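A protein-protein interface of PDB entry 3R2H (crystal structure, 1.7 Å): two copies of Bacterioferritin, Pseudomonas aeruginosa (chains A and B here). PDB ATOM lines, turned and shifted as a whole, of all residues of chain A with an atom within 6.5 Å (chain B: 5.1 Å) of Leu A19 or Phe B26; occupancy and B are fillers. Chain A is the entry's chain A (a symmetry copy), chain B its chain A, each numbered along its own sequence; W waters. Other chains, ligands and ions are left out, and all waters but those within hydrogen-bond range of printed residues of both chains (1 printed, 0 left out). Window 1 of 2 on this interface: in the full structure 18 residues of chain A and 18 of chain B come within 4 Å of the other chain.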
ATOM      1  N   LEU A  14      -0.726 -11.723  26.786  1.00  0.00           N
ATOM      2  CA  LEU A  14       0.198 -12.364  25.862  1.00  0.00           C
ATOM      3  C   LEU A  14       0.785 -11.347  24.881  1.00  0.00           C
ATOM      4  O   LEU A  14       1.984 -11.403  24.557  1.00  0.00           O
ATOM      5  CB  LEU A  14      -0.523 -13.479  25.087  1.00  0.00           C
ATOM      6  CG  LEU A  14      -0.922 -14.672  25.968  1.00  0.00           C
ATOM      7  CD1 LEU A  14      -1.793 -15.676  25.203  1.00  0.00           C
ATOM      8  CD2 LEU A  14       0.306 -15.375  26.493  1.00  0.00           C
ATOM      9  N   LEU A  15      -0.047 -10.414  24.418  1.00  0.00           N
ATOM     10  CA  LEU A  15       0.415  -9.394  23.459  1.00  0.00           C
ATOM     11  C   LEU A  15       1.568  -8.566  24.032  1.00  0.00           C
ATOM     12  O   LEU A  15       2.575  -8.358  23.343  1.00  0.00           O
ATOM     13  CB  LEU A  15      -0.730  -8.446  23.040  1.00  0.00           C
ATOM     14  CG  LEU A  15      -0.324  -7.237  22.175  1.00  0.00           C
ATOM     15  CD1 LEU A  15       0.386  -7.700  20.887  1.00  0.00           C
ATOM     16  CD2 LEU A  15      -1.564  -6.427  21.805  1.00  0.00           C
ATOM     17  N   THR A  16       1.422  -8.051  25.259  1.00  0.00           N
ATOM     18  CA  THR A  16       2.510  -7.239  25.818  1.00  0.00           C
ATOM     19  C   THR A  16       3.767  -8.092  26.010  1.00  0.00           C
ATOM     20  O   THR A  16       4.885  -7.594  25.916  1.00  0.00           O
ATOM     21  CB  THR A  16       2.095  -6.521  27.143  1.00  0.00           C
ATOM     22  OG1 THR A  16       1.777  -7.490  28.160  1.00  0.00           O
ATOM     23  CG2 THR A  16       0.873  -5.609  26.899  1.00  0.00           C
ATOM     24  N   GLY A  17       3.593  -9.375  26.285  1.00  0.00           N
ATOM     25  CA  GLY A  17       4.729 -10.298  26.354  1.00  0.00           C
ATOM     26  C   GLY A  17       5.425 -10.476  25.009  1.00  0.00           C
ATOM     27  O   GLY A  17       6.657 -10.585  24.960  1.00  0.00           O
ATOM     28  N   GLU A  18       4.665 -10.543  23.921  1.00  0.00           N
ATOM     29  CA  GLU A  18       5.276 -10.781  22.607  1.00  0.00           C
ATOM     30  C   GLU A  18       5.930  -9.499  22.092  1.00  0.00           C
ATOM     31  O   GLU A  18       6.952  -9.555  21.426  1.00  0.00           O
ATOM     32  CB  GLU A  18       4.252 -11.255  21.553  1.00  0.00           C
ATOM     33  CG  GLU A  18       3.478 -12.508  21.911  1.00  0.00           C
ATOM     34  CD  GLU A  18       4.338 -13.695  22.232  1.00  0.00           C
ATOM     35  OE1 GLU A  18       5.427 -13.826  21.642  1.00  0.00           O
ATOM     36  OE2 GLU A  18       3.896 -14.512  23.073  1.00  0.00           O
ATOM     37  N   LEU A  19       5.337  -8.353  22.375  1.00  0.00           N
ATOM     38  CA  LEU A  19       5.958  -7.062  22.027  1.00  0.00           C
ATOM     39  C   LEU A  19       7.326  -6.942  22.731  1.00  0.00           C
ATOM     40  O   LEU A  19       8.306  -6.503  22.157  1.00  0.00           O
ATOM     41  CB  LEU A  19       5.046  -5.892  22.430  1.00  0.00           C
ATOM     42  CG  LEU A  19       3.744  -5.855  21.610  1.00  0.00           C
ATOM     43  CD1 LEU A  19       2.810  -4.821  22.224  1.00  0.00           C
ATOM     44  CD2 LEU A  19       4.003  -5.511  20.116  1.00  0.00           C
ATOM     45  N   ALA A  20       7.386  -7.391  23.976  1.00  0.00           N
ATOM     46  CA  ALA A  20       8.646  -7.377  24.712  1.00  0.00           C
ATOM     47  C   ALA A  20       9.641  -8.384  24.139  1.00  0.00           C
ATOM     48  O   ALA A  20      10.825  -8.065  23.958  1.00  0.00           O
ATOM     49  CB  ALA A  20       8.385  -7.666  26.178  1.00  0.00           C
ATOM     50  N   ALA A  21       9.192  -9.607  23.852  1.00  0.00           N
ATOM     51  CA  ALA A  21      10.114 -10.608  23.291  1.00  0.00           C
ATOM     52  C   ALA A  21      10.720 -10.094  21.954  1.00  0.00           C
ATOM     53  O   ALA A  21      11.931 -10.192  21.727  1.00  0.00           O
ATOM     54  CB  ALA A  21       9.388 -11.905  23.089  1.00  0.00           C
ATOM     55  N   ARG A  22       9.870  -9.526  21.094  1.00  0.00           N
ATOM     56  CA  ARG A  22      10.319  -8.896  19.845  1.00  0.00           C
ATOM     57  C   ARG A  22      11.489  -7.930  20.141  1.00  0.00           C
ATOM     58  O   ARG A  22      12.517  -7.937  19.468  1.00  0.00           O
ATOM     59  CB  ARG A  22       9.130  -8.136  19.227  1.00  0.00           C
ATOM     60  CG  ARG A  22       9.528  -7.093  18.168  1.00  0.00           C
ATOM     61  CD  ARG A  22       8.384  -6.069  17.920  1.00  0.00           C
ATOM     62  NE  ARG A  22       8.117  -5.294  19.135  1.00  0.00           N
ATOM     63  CZ  ARG A  22       7.299  -4.250  19.205  1.00  0.00           C
ATOM     64  NH1 ARG A  22       6.637  -3.838  18.124  1.00  0.00           N
ATOM     65  NH2 ARG A  22       7.158  -3.614  20.361  1.00  0.00           N
ATOM     66  N   ASP A  23      11.322  -7.080  21.146  1.00  0.00           N
ATOM     67  CA  ASP A  23      12.323  -6.073  21.444  1.00  0.00           C
ATOM     68  C   ASP A  23      13.558  -6.643  22.110  1.00  0.00           C
ATOM     69  O   ASP A  23      14.672  -6.147  21.877  1.00  0.00           O
ATOM     70  CB  ASP A  23      11.703  -4.946  22.282  1.00  0.00           C
ATOM     71  CG  ASP A  23      10.765  -4.069  21.450  1.00  0.00           C
ATOM     72  OD1 ASP A  23      10.883  -4.113  20.207  1.00  0.00           O
ATOM     73  OD2 ASP A  23       9.939  -3.352  22.021  1.00  0.00           O
ATOM     74  N   GLN A  24      13.403  -7.699  22.905  1.00  0.00           N
ATOM     75  CA  GLN A  24      14.603  -8.322  23.475  1.00  0.00           C
ATOM     76  C   GLN A  24      15.415  -8.965  22.353  1.00  0.00           C
ATOM     77  O   GLN A  24      16.634  -8.950  22.389  1.00  0.00           O
ATOM     78  CB  GLN A  24      14.228  -9.359  24.532  1.00  0.00           C
ATOM     79  CG  GLN A  24      15.473  -9.993  25.229  1.00  0.00           C
ATOM     80  CD  GLN A  24      15.093 -10.604  26.558  1.00  0.00           C
ATOM     81  OE1 GLN A  24      14.493  -9.949  27.406  1.00  0.00           O
ATOM     82  NE2 GLN A  24      15.422 -11.881  26.743  1.00  0.00           N
ATOM     83  N   GLU A  51       8.490 -12.995  16.314  1.00  0.00           N
ATOM     84  CA  GLU A  51       7.760 -12.403  17.431  1.00  0.00           C
ATOM     85  C   GLU A  51       6.846 -11.288  16.960  1.00  0.00           C
ATOM     86  O   GLU A  51       5.771 -11.133  17.499  1.00  0.00           O
ATOM     87  CB  GLU A  51       8.707 -11.829  18.485  1.00  0.00           C
ATOM     88  CG  GLU A  51       9.277 -12.882  19.360  1.00  0.00           C
ATOM     89  CD  GLU A  51       8.182 -13.600  20.104  1.00  0.00           C
ATOM     90  OE1 GLU A  51       7.246 -12.944  20.594  1.00  0.00           O
ATOM     91  OE2 GLU A  51       8.239 -14.807  20.166  1.00  0.00           O
ATOM     92  N   THR A  52       7.282 -10.506  15.981  1.00  0.00           N
ATOM     93  CA  THR A  52       6.434  -9.457  15.425  1.00  0.00           C
ATOM     94  C   THR A  52       5.192 -10.107  14.807  1.00  0.00           C
ATOM     95  O   THR A  52       4.085  -9.624  14.992  1.00  0.00           O
ATOM     96  CB  THR A  52       7.198  -8.605  14.410  1.00  0.00           C
ATOM     97  OG1 THR A  52       8.342  -8.011  15.066  1.00  0.00           O
ATOM     98  CG2 THR A  52       6.312  -7.509  13.826  1.00  0.00           C
ATOM     99  N   GLN A  53       5.370 -11.212  14.094  1.00  0.00           N
ATOM    100  CA  GLN A  53       4.213 -11.922  13.553  1.00  0.00           C
ATOM    101  C   GLN A  53       3.318 -12.472  14.661  1.00  0.00           C
ATOM    102  O   GLN A  53       2.101 -12.407  14.521  1.00  0.00           O
ATOM    103  CB  GLN A  53       4.680 -13.055  12.635  1.00  0.00           C
ATOM    104  CG  GLN A  53       5.343 -12.459  11.393  1.00  0.00           C
ATOM    105  CD  GLN A  53       5.870 -13.494  10.407  1.00  0.00           C
ATOM    106  OE1 GLN A  53       5.443 -14.649  10.407  1.00  0.00           O
ATOM    107  NE2 GLN A  53       6.811 -13.073   9.557  1.00  0.00           N
ATOM    108  N   ALA A  55       2.903 -11.222  17.701  1.00  0.00           N
ATOM    109  CA  ALA A  55       2.230 -10.040  18.268  1.00  0.00           C
ATOM    110  C   ALA A  55       1.120  -9.609  17.335  1.00  0.00           C
ATOM    111  O   ALA A  55       0.030  -9.327  17.779  1.00  0.00           O
ATOM    112  CB  ALA A  55       3.228  -8.884  18.451  1.00  0.00           C
ATOM    113  N   ASP A  56       1.399  -9.562  16.030  1.00  0.00           N
ATOM    114  CA  ASP A  56       0.390  -9.144  15.046  1.00  0.00           C
ATOM    115  C   ASP A  56      -0.832 -10.056  15.111  1.00  0.00           C
ATOM    116  O   ASP A  56      -1.968  -9.588  15.097  1.00  0.00           O
ATOM    117  CB  ASP A  56       1.008  -9.191  13.635  1.00  0.00           C
ATOM    118  CG  ASP A  56       0.189  -8.433  12.590  1.00  0.00           C
ATOM    119  OD1 ASP A  56      -0.689  -7.617  12.951  1.00  0.00           O
ATOM    120  OD2 ASP A  56       0.491  -8.610  11.376  1.00  0.00           O
ATOM    121  N   ALA A  57      -0.616 -11.370  15.173  1.00  0.00           N
ATOM    122  CA  ALA A  57      -1.754 -12.307  15.237  1.00  0.00           C
ATOM    123  C   ALA A  57      -2.619 -12.031  16.471  1.00  0.00           C
ATOM    124  O   ALA A  57      -3.854 -12.045  16.396  1.00  0.00           O
ATOM    125  CB  ALA A  57      -1.241 -13.753  15.268  1.00  0.00           C
ATOM    126  N   LEU A  59      -2.793  -9.133  18.317  1.00  0.00           N
ATOM    127  CA  LEU A  59      -3.402  -7.822  18.158  1.00  0.00           C
ATOM    128  C   LEU A  59      -4.634  -7.901  17.252  1.00  0.00           C
ATOM    129  O   LEU A  59      -5.702  -7.391  17.595  1.00  0.00           O
ATOM    130  CB  LEU A  59      -2.337  -6.876  17.582  1.00  0.00           C
ATOM    131  CG  LEU A  59      -2.607  -5.369  17.555  1.00  0.00           C
ATOM    132  CD1 LEU A  59      -1.324  -4.679  17.171  1.00  0.00           C
ATOM    133  CD2 LEU A  59      -3.658  -5.040  16.572  1.00  0.00           C
ATOM    134  N   ARG A  60      -4.507  -8.564  16.106  1.00  0.00           N
ATOM    135  CA  ARG A  60      -5.632  -8.629  15.189  1.00  0.00           C
ATOM    136  C   ARG A  60      -6.794  -9.399  15.779  1.00  0.00           C
ATOM    137  O   ARG A  60      -7.945  -9.048  15.548  1.00  0.00           O
ATOM    138  CB  ARG A  60      -5.218  -9.285  13.887  1.00  0.00           C
ATOM    139  CG  ARG A  60      -4.357  -8.349  13.014  1.00  0.00           C
ATOM    140  CD  ARG A  60      -3.906  -9.118  11.810  1.00  0.00           C
ATOM    141  NE  ARG A  60      -2.878  -8.431  11.047  1.00  0.00           N
ATOM    142  CZ  ARG A  60      -3.074  -7.889   9.864  1.00  0.00           C
ATOM    143  NH1 ARG A  60      -4.266  -7.932   9.316  1.00  0.00           N
ATOM    144  NH2 ARG A  60      -2.069  -7.319   9.226  1.00  0.00           N
ATOM    145  N   ARG A  70      -3.512  -3.738  24.249  1.00  0.00           N
ATOM    146  CA  ARG A  70      -2.566  -3.050  25.119  1.00  0.00           C
ATOM    147  C   ARG A  70      -1.216  -3.077  24.447  1.00  0.00           C
ATOM    148  O   ARG A  70      -0.695  -4.143  24.205  1.00  0.00           O
ATOM    149  CB  ARG A  70      -2.467  -3.759  26.478  1.00  0.00           C
ATOM    150  CG  ARG A  70      -3.696  -3.570  27.337  1.00  0.00           C
ATOM    151  CD  ARG A  70      -3.363  -3.673  28.808  1.00  0.00           C
ATOM    152  NE  ARG A  70      -2.957  -5.013  29.210  1.00  0.00           N
ATOM    153  CZ  ARG A  70      -3.795  -5.965  29.608  1.00  0.00           C
ATOM    154  NH1 ARG A  70      -5.112  -5.763  29.622  1.00  0.00           N
ATOM    155  NH2 ARG A  70      -3.319  -7.145  29.974  1.00  0.00           N
ATOM    156  N   MET A  71      -0.650  -1.912  24.146  1.00  0.00           N
ATOM    157  CA  MET A  71       0.574  -1.859  23.324  1.00  0.00           C
ATOM    158  C   MET A  71       1.841  -1.583  24.131  1.00  0.00           C
ATOM    159  O   MET A  71       2.919  -1.477  23.566  1.00  0.00           O
ATOM    160  CB  MET A  71       0.433  -0.780  22.231  1.00  0.00           C
ATOM    161  CG  MET A  71      -0.713  -1.074  21.246  1.00  0.00           C
ATOM    162  SD  MET A  71      -0.483  -2.614  20.318  1.00  0.00           S
ATOM    163  CE  MET A  71       1.016  -2.232  19.411  1.00  0.00           C
ATOM    164  N   ARG A  72       1.734  -1.446  25.454  1.00  0.00           N
ATOM    165  CA  ARG A  72       2.959  -1.253  26.253  1.00  0.00           C
ATOM    166  C   ARG A  72       3.703  -2.573  26.422  1.00  0.00           C
ATOM    167  O   ARG A  72       3.192  -3.495  27.048  1.00  0.00           O
ATOM    168  CB  ARG A  72       2.605  -0.714  27.646  1.00  0.00           C
ATOM    169  CG  ARG A  72       3.845  -0.404  28.447  1.00  0.00           C
ATOM    170  CD  ARG A  72       3.465   0.215  29.801  1.00  0.00           C
ATOM    171  NE  ARG A  72       3.193  -0.872  30.709  1.00  0.00           N
ATOM    172  CZ  ARG A  72       3.144  -0.753  32.036  1.00  0.00           C
ATOM    173  NH1 ARG A  72       3.344   0.425  32.614  1.00  0.00           N
ATOM    174  NH2 ARG A  72       2.899  -1.825  32.776  1.00  0.00           N
ATOM    175  N   PRO A  73       4.920  -2.691  25.872  1.00  0.00           N
ATOM    176  CA  PRO A  73       5.612  -3.982  26.046  1.00  0.00           C
ATOM    177  C   PRO A  73       5.959  -4.245  27.492  1.00  0.00           C
ATOM    178  O   PRO A  73       6.173  -3.281  28.224  1.00  0.00           O
ATOM    179  CB  PRO A  73       6.904  -3.825  25.202  1.00  0.00           C
ATOM    180  CG  PRO A  73       6.572  -2.671  24.217  1.00  0.00           C
ATOM    181  CD  PRO A  73       5.695  -1.749  25.036  1.00  0.00           C
ATOM    182  N   ASP A  74       6.008  -5.515  27.902  1.00  0.00           N
ATOM    183  CA  ASP A  74       6.567  -5.851  29.217  1.00  0.00           C
ATOM    184  C   ASP A  74       8.037  -5.404  29.264  1.00  0.00           C
ATOM    185  O   ASP A  74       8.670  -5.175  28.226  1.00  0.00           O
ATOM    186  CB  ASP A  74       6.513  -7.366  29.466  1.00  0.00           C
ATOM    187  CG  ASP A  74       5.106  -7.920  29.504  1.00  0.00           C
ATOM    188  OD1 ASP A  74       4.154  -7.138  29.598  1.00  0.00           O
ATOM    189  OD2 ASP A  74       4.956  -9.166  29.494  1.00  0.00           O
ATOM    190  N   ILE A  76      11.999  -5.789  29.380  1.00  0.00           N
ATOM    191  CA  ILE A  76      12.918  -6.803  28.881  1.00  0.00           C
ATOM    192  C   ILE A  76      14.146  -6.880  29.786  1.00  0.00           C
ATOM    193  O   ILE A  76      14.377  -5.987  30.621  1.00  0.00           O
ATOM    194  CB  ILE A  76      13.332  -6.568  27.407  1.00  0.00           C
ATOM    195  CG1 ILE A  76      14.088  -5.254  27.249  1.00  0.00           C
ATOM    196  CG2 ILE A  76      12.080  -6.545  26.498  1.00  0.00           C
ATOM    197  CD1 ILE A  76      14.847  -5.169  25.915  1.00  0.00           C
ATOM    198  N   ALA B  21       6.806   5.253  18.154  1.00  0.00           N
ATOM    199  CA  ALA B  21       6.126   5.595  16.894  1.00  0.00           C
ATOM    200  C   ALA B  21       5.806   4.304  16.088  1.00  0.00           C
ATOM    201  O   ALA B  21       4.694   4.136  15.577  1.00  0.00           O
ATOM    202  CB  ALA B  21       6.986   6.530  16.096  1.00  0.00           C
ATOM    203  N   ARG B  22       6.781   3.395  16.005  1.00  0.00           N
ATOM    204  CA  ARG B  22       6.583   2.084  15.373  1.00  0.00           C
ATOM    205  C   ARG B  22       5.299   1.427  15.930  1.00  0.00           C
ATOM    206  O   ARG B  22       4.460   0.922  15.188  1.00  0.00           O
ATOM    207  CB  ARG B  22       7.815   1.207  15.669  1.00  0.00           C
ATOM    208  CG  ARG B  22       7.587  -0.298  15.449  1.00  0.00           C
ATOM    209  CD  ARG B  22       8.668  -1.148  16.176  1.00  0.00           C
ATOM    210  NE  ARG B  22       8.579  -0.959  17.627  1.00  0.00           N
ATOM    211  CZ  ARG B  22       9.269  -1.651  18.526  1.00  0.00           C
ATOM    212  NH1 ARG B  22      10.126  -2.595  18.139  1.00  0.00           N
ATOM    213  NH2 ARG B  22       9.084  -1.402  19.817  1.00  0.00           N
ATOM    214  N   ASP B  23       5.157   1.419  17.249  1.00  0.00           N
ATOM    215  CA  ASP B  23       4.034   0.745  17.872  1.00  0.00           C
ATOM    216  C   ASP B  23       2.730   1.501  17.720  1.00  0.00           C
ATOM    217  O   ASP B  23       1.663   0.878  17.602  1.00  0.00           O
ATOM    218  CB  ASP B  23       4.346   0.455  19.347  1.00  0.00           C
ATOM    219  CG  ASP B  23       5.373  -0.667  19.501  1.00  0.00           C
ATOM    220  OD1 ASP B  23       5.551  -1.426  18.525  1.00  0.00           O
ATOM    221  OD2 ASP B  23       5.981  -0.792  20.567  1.00  0.00           O
ATOM    222  N   GLN B  24       2.785   2.830  17.679  1.00  0.00           N
ATOM    223  CA  GLN B  24       1.542   3.569  17.431  1.00  0.00           C
ATOM    224  C   GLN B  24       1.069   3.290  16.006  1.00  0.00           C
ATOM    225  O   GLN B  24      -0.122   3.200  15.760  1.00  0.00           O
ATOM    226  CB  GLN B  24       1.747   5.067  17.647  1.00  0.00           C
ATOM    227  CG  GLN B  24       0.432   5.892  17.476  1.00  0.00           C
ATOM    228  CD  GLN B  24       0.543   7.233  18.164  1.00  0.00           C
ATOM    229  OE1 GLN B  24       0.874   7.312  19.344  1.00  0.00           O
ATOM    230  NE2 GLN B  24       0.289   8.307  17.420  1.00  0.00           N
ATOM    231  N   TYR B  25       1.989   3.179  15.047  1.00  0.00           N
ATOM    232  CA  TYR B  25       1.539   2.883  13.672  1.00  0.00           C
ATOM    233  C   TYR B  25       1.127   1.416  13.514  1.00  0.00           C
ATOM    234  O   TYR B  25       0.282   1.108  12.686  1.00  0.00           O
ATOM    235  CB  TYR B  25       2.643   3.257  12.651  1.00  0.00           C
ATOM    236  CG  TYR B  25       3.113   4.695  12.822  1.00  0.00           C
ATOM    237  CD1 TYR B  25       2.301   5.643  13.457  1.00  0.00           C
ATOM    238  CD2 TYR B  25       4.369   5.093  12.403  1.00  0.00           C
ATOM    239  CE1 TYR B  25       2.731   6.947  13.649  1.00  0.00           C
ATOM    240  CE2 TYR B  25       4.815   6.404  12.597  1.00  0.00           C
ATOM    241  CZ  TYR B  25       3.980   7.322  13.241  1.00  0.00           C
ATOM    242  OH  TYR B  25       4.371   8.642  13.474  1.00  0.00           O
ATOM    243  N   PHE B  26       1.698   0.523  14.328  1.00  0.00           N
ATOM    244  CA  PHE B  26       1.272  -0.888  14.414  1.00  0.00           C
ATOM    245  C   PHE B  26      -0.206  -0.927  14.811  1.00  0.00           C
ATOM    246  O   PHE B  26      -1.032  -1.507  14.111  1.00  0.00           O
ATOM    247  CB  PHE B  26       2.161  -1.573  15.477  1.00  0.00           C
ATOM    248  CG  PHE B  26       2.181  -3.105  15.468  1.00  0.00           C
ATOM    249  CD1 PHE B  26       2.995  -3.760  16.382  1.00  0.00           C
ATOM    250  CD2 PHE B  26       1.413  -3.873  14.597  1.00  0.00           C
ATOM    251  CE1 PHE B  26       3.082  -5.151  16.408  1.00  0.00           C
ATOM    252  CE2 PHE B  26       1.495  -5.270  14.620  1.00  0.00           C
ATOM    253  CZ  PHE B  26       2.316  -5.908  15.505  1.00  0.00           C
ATOM    254  N   ILE B  27      -0.572  -0.297  15.925  1.00  0.00           N
ATOM    255  CA  ILE B  27      -1.965  -0.379  16.347  1.00  0.00           C
ATOM    256  C   ILE B  27      -2.882   0.378  15.393  1.00  0.00           C
ATOM    257  O   ILE B  27      -3.924  -0.141  15.010  1.00  0.00           O
ATOM    258  CB  ILE B  27      -2.190   0.046  17.843  1.00  0.00           C
ATOM    259  CG1 ILE B  27      -3.658  -0.087  18.229  1.00  0.00           C
ATOM    260  CG2 ILE B  27      -1.728   1.478  18.141  1.00  0.00           C
ATOM    261  CD1 ILE B  27      -4.202  -1.453  18.050  1.00  0.00           C
ATOM    262  N   HIS B  28      -2.512   1.583  14.965  1.00  0.00           N
ATOM    263  CA  HIS B  28      -3.400   2.307  14.015  1.00  0.00           C
ATOM    264  C   HIS B  28      -3.601   1.550  12.690  1.00  0.00           C
ATOM    265  O   HIS B  28      -4.718   1.460  12.213  1.00  0.00           O
ATOM    266  CB  HIS B  28      -2.867   3.709  13.699  1.00  0.00           C
ATOM    267  CG  HIS B  28      -3.125   4.719  14.785  1.00  0.00           C
ATOM    268  ND1 HIS B  28      -2.543   5.970  14.783  1.00  0.00           N
ATOM    269  CD2 HIS B  28      -3.905   4.663  15.892  1.00  0.00           C
ATOM    270  CE1 HIS B  28      -2.965   6.649  15.840  1.00  0.00           C
ATOM    271  NE2 HIS B  28      -3.785   5.879  16.529  1.00  0.00           N
ATOM    272  N   SER B  29      -2.542   0.997  12.103  1.00  0.00           N
ATOM    273  CA  SER B  29      -2.724   0.293  10.834  1.00  0.00           C
ATOM    274  C   SER B  29      -3.728  -0.848  11.011  1.00  0.00           C
ATOM    275  O   SER B  29      -4.622  -1.042  10.174  1.00  0.00           O
ATOM    276  CB  SER B  29      -1.378  -0.217  10.301  1.00  0.00           C
ATOM    277  OG  SER B  29      -0.780  -1.122  11.192  1.00  0.00           O
ATOM    278  N   ARG B  30      -3.617  -1.603  12.104  1.00  0.00           N
ATOM    279  CA  ARG B  30      -4.519  -2.740  12.291  1.00  0.00           C
ATOM    280  C   ARG B  30      -5.941  -2.293  12.636  1.00  0.00           C
ATOM    281  O   ARG B  30      -6.897  -2.974  12.262  1.00  0.00           O
ATOM    282  CB  ARG B  30      -3.971  -3.698  13.328  1.00  0.00           C
ATOM    283  CG  ARG B  30      -2.998  -4.735  12.718  1.00  0.00           C
ATOM    284  CD  ARG B  30      -1.743  -4.111  12.135  1.00  0.00           C
ATOM    285  NE  ARG B  30      -0.812  -5.155  11.684  1.00  0.00           N
ATOM    286  CZ  ARG B  30       0.235  -4.904  10.908  1.00  0.00           C
ATOM    287  NH1 ARG B  30       0.475  -3.659  10.488  1.00  0.00           N
ATOM    288  NH2 ARG B  30       1.051  -5.887  10.552  1.00  0.00           N
ATOM    289  N   MET B  48       4.948   2.025   9.886  1.00  0.00           N
ATOM    290  CA  MET B  48       5.488   1.161  10.950  1.00  0.00           C
ATOM    291  C   MET B  48       6.822   0.528  10.564  1.00  0.00           C
ATOM    292  O   MET B  48       7.771   0.536  11.363  1.00  0.00           O
ATOM    293  CB  MET B  48       4.516   0.022  11.266  1.00  0.00           C
ATOM    294  CG  MET B  48       5.063  -0.895  12.349  1.00  0.00           C
ATOM    295  SD  MET B  48       3.979  -2.337  12.594  1.00  0.00           S
ATOM    296  CE  MET B  48       4.246  -3.249  11.068  1.00  0.00           C
HETATM  297  O   HOH W   1       4.722   0.411  22.548  1.00  0.00           O
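NH1 of Arg B22 is in salt-bridge range of OD1 of Asp A23 (2.7 Å). The side-chain carboxylate (OD1) of Asp B23 lies within salt-bridge range of the guanidinium group (NH1) of Arg A22 (2.7 Å). The guanidinium group (NE) of Arg B30 lies within salt-bridge range of the side-chain carboxylate (OD1) of Asp A56 (2.8 Å). NH2 of Arg A22 lies close to NH2 of Arg B22, 3.0 Å away.
Among the printed residues, 13 pairs touch across the chains.
Leu A19 touches Phe B26 (CD2 to CE1, 3.8 Å). Phe B26 touches Asp A56. CD1 of Leu A59 touches CD2 of Phe B26 (3.8 Å). CD1 of Ile B27 touches CD2 of Leu A59 (3.9 Å). Arg B30 touches Leu A59 (CB to CD2, 3.5 Å). Arg B30 touches Arg A60 (NE to NH2, 3.5 Å). O of Asp B23 touches CE of Met A71, 3.7 Å away. Met A71 touches Phe B26. CG of Met A71 touches CB of Ile B27, 3.9 Å away.
Leu A19 touches just one residue of chain B: Phe B26. Phe B26 touches four residues of chain A. Of the printed residues of chain B, Asp A23 touches Arg B22 (2.7 Å). Printed residues of chain B within 4 Å of Met A71: Asp B23 (3.7 Å), Phe B26 (3.9 Å) and Ile B27 (3.9 Å). The nearest residue of chain B that does not touch Leu A19 is Asp B23 (4.6 Å). The nearest residue of chain A that does not touch Phe B26 is Arg A22 (4.04 Å). The nearest printed residue of chain A that does not touch Arg B30 is Thr A52 (6.4 Å).
Arg A22 touches its own counterpart, Arg B22. Arg A22 touches Asp B23, and with the chains exchanged Asp A23 touches Arg B22. 4 positions are printed for both chains. Of the 13 pairs that touch across the chains among the printed residues, 3 have their exchanged pair printed and touching as well.
Water W1 lies within hydrogen-bond range of OD2 of Asp B23 and O of Met A71.
The guanidinium group (NE) of Arg B22 lies within salt-bridge range of the side-chain carboxylate (OD1) of Asp B23 (3.2 Å). O of Phe B26 sits at hydrogen-bond distance from OG of Ser B29 (3.0 Å). The side-chain hydroxyl of Ser B29 sits at hydrogen-bond distance from the guanidinium group of Arg B30. The backbone carbonyl oxygen (O) of Leu A19 lies within hydrogen-bond range of the guanidinium group (NE) of Arg A22. The guanidinium group (NE) of Arg A22 lies within salt-bridge range of the side-chain carboxylate (OD1) of Asp A23 (3.2 Å). The side-chain carboxylate (OD1) of Asp A56 lies within salt-bridge range of the guanidinium group (NE) of Arg A60, at 3.0 Å.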
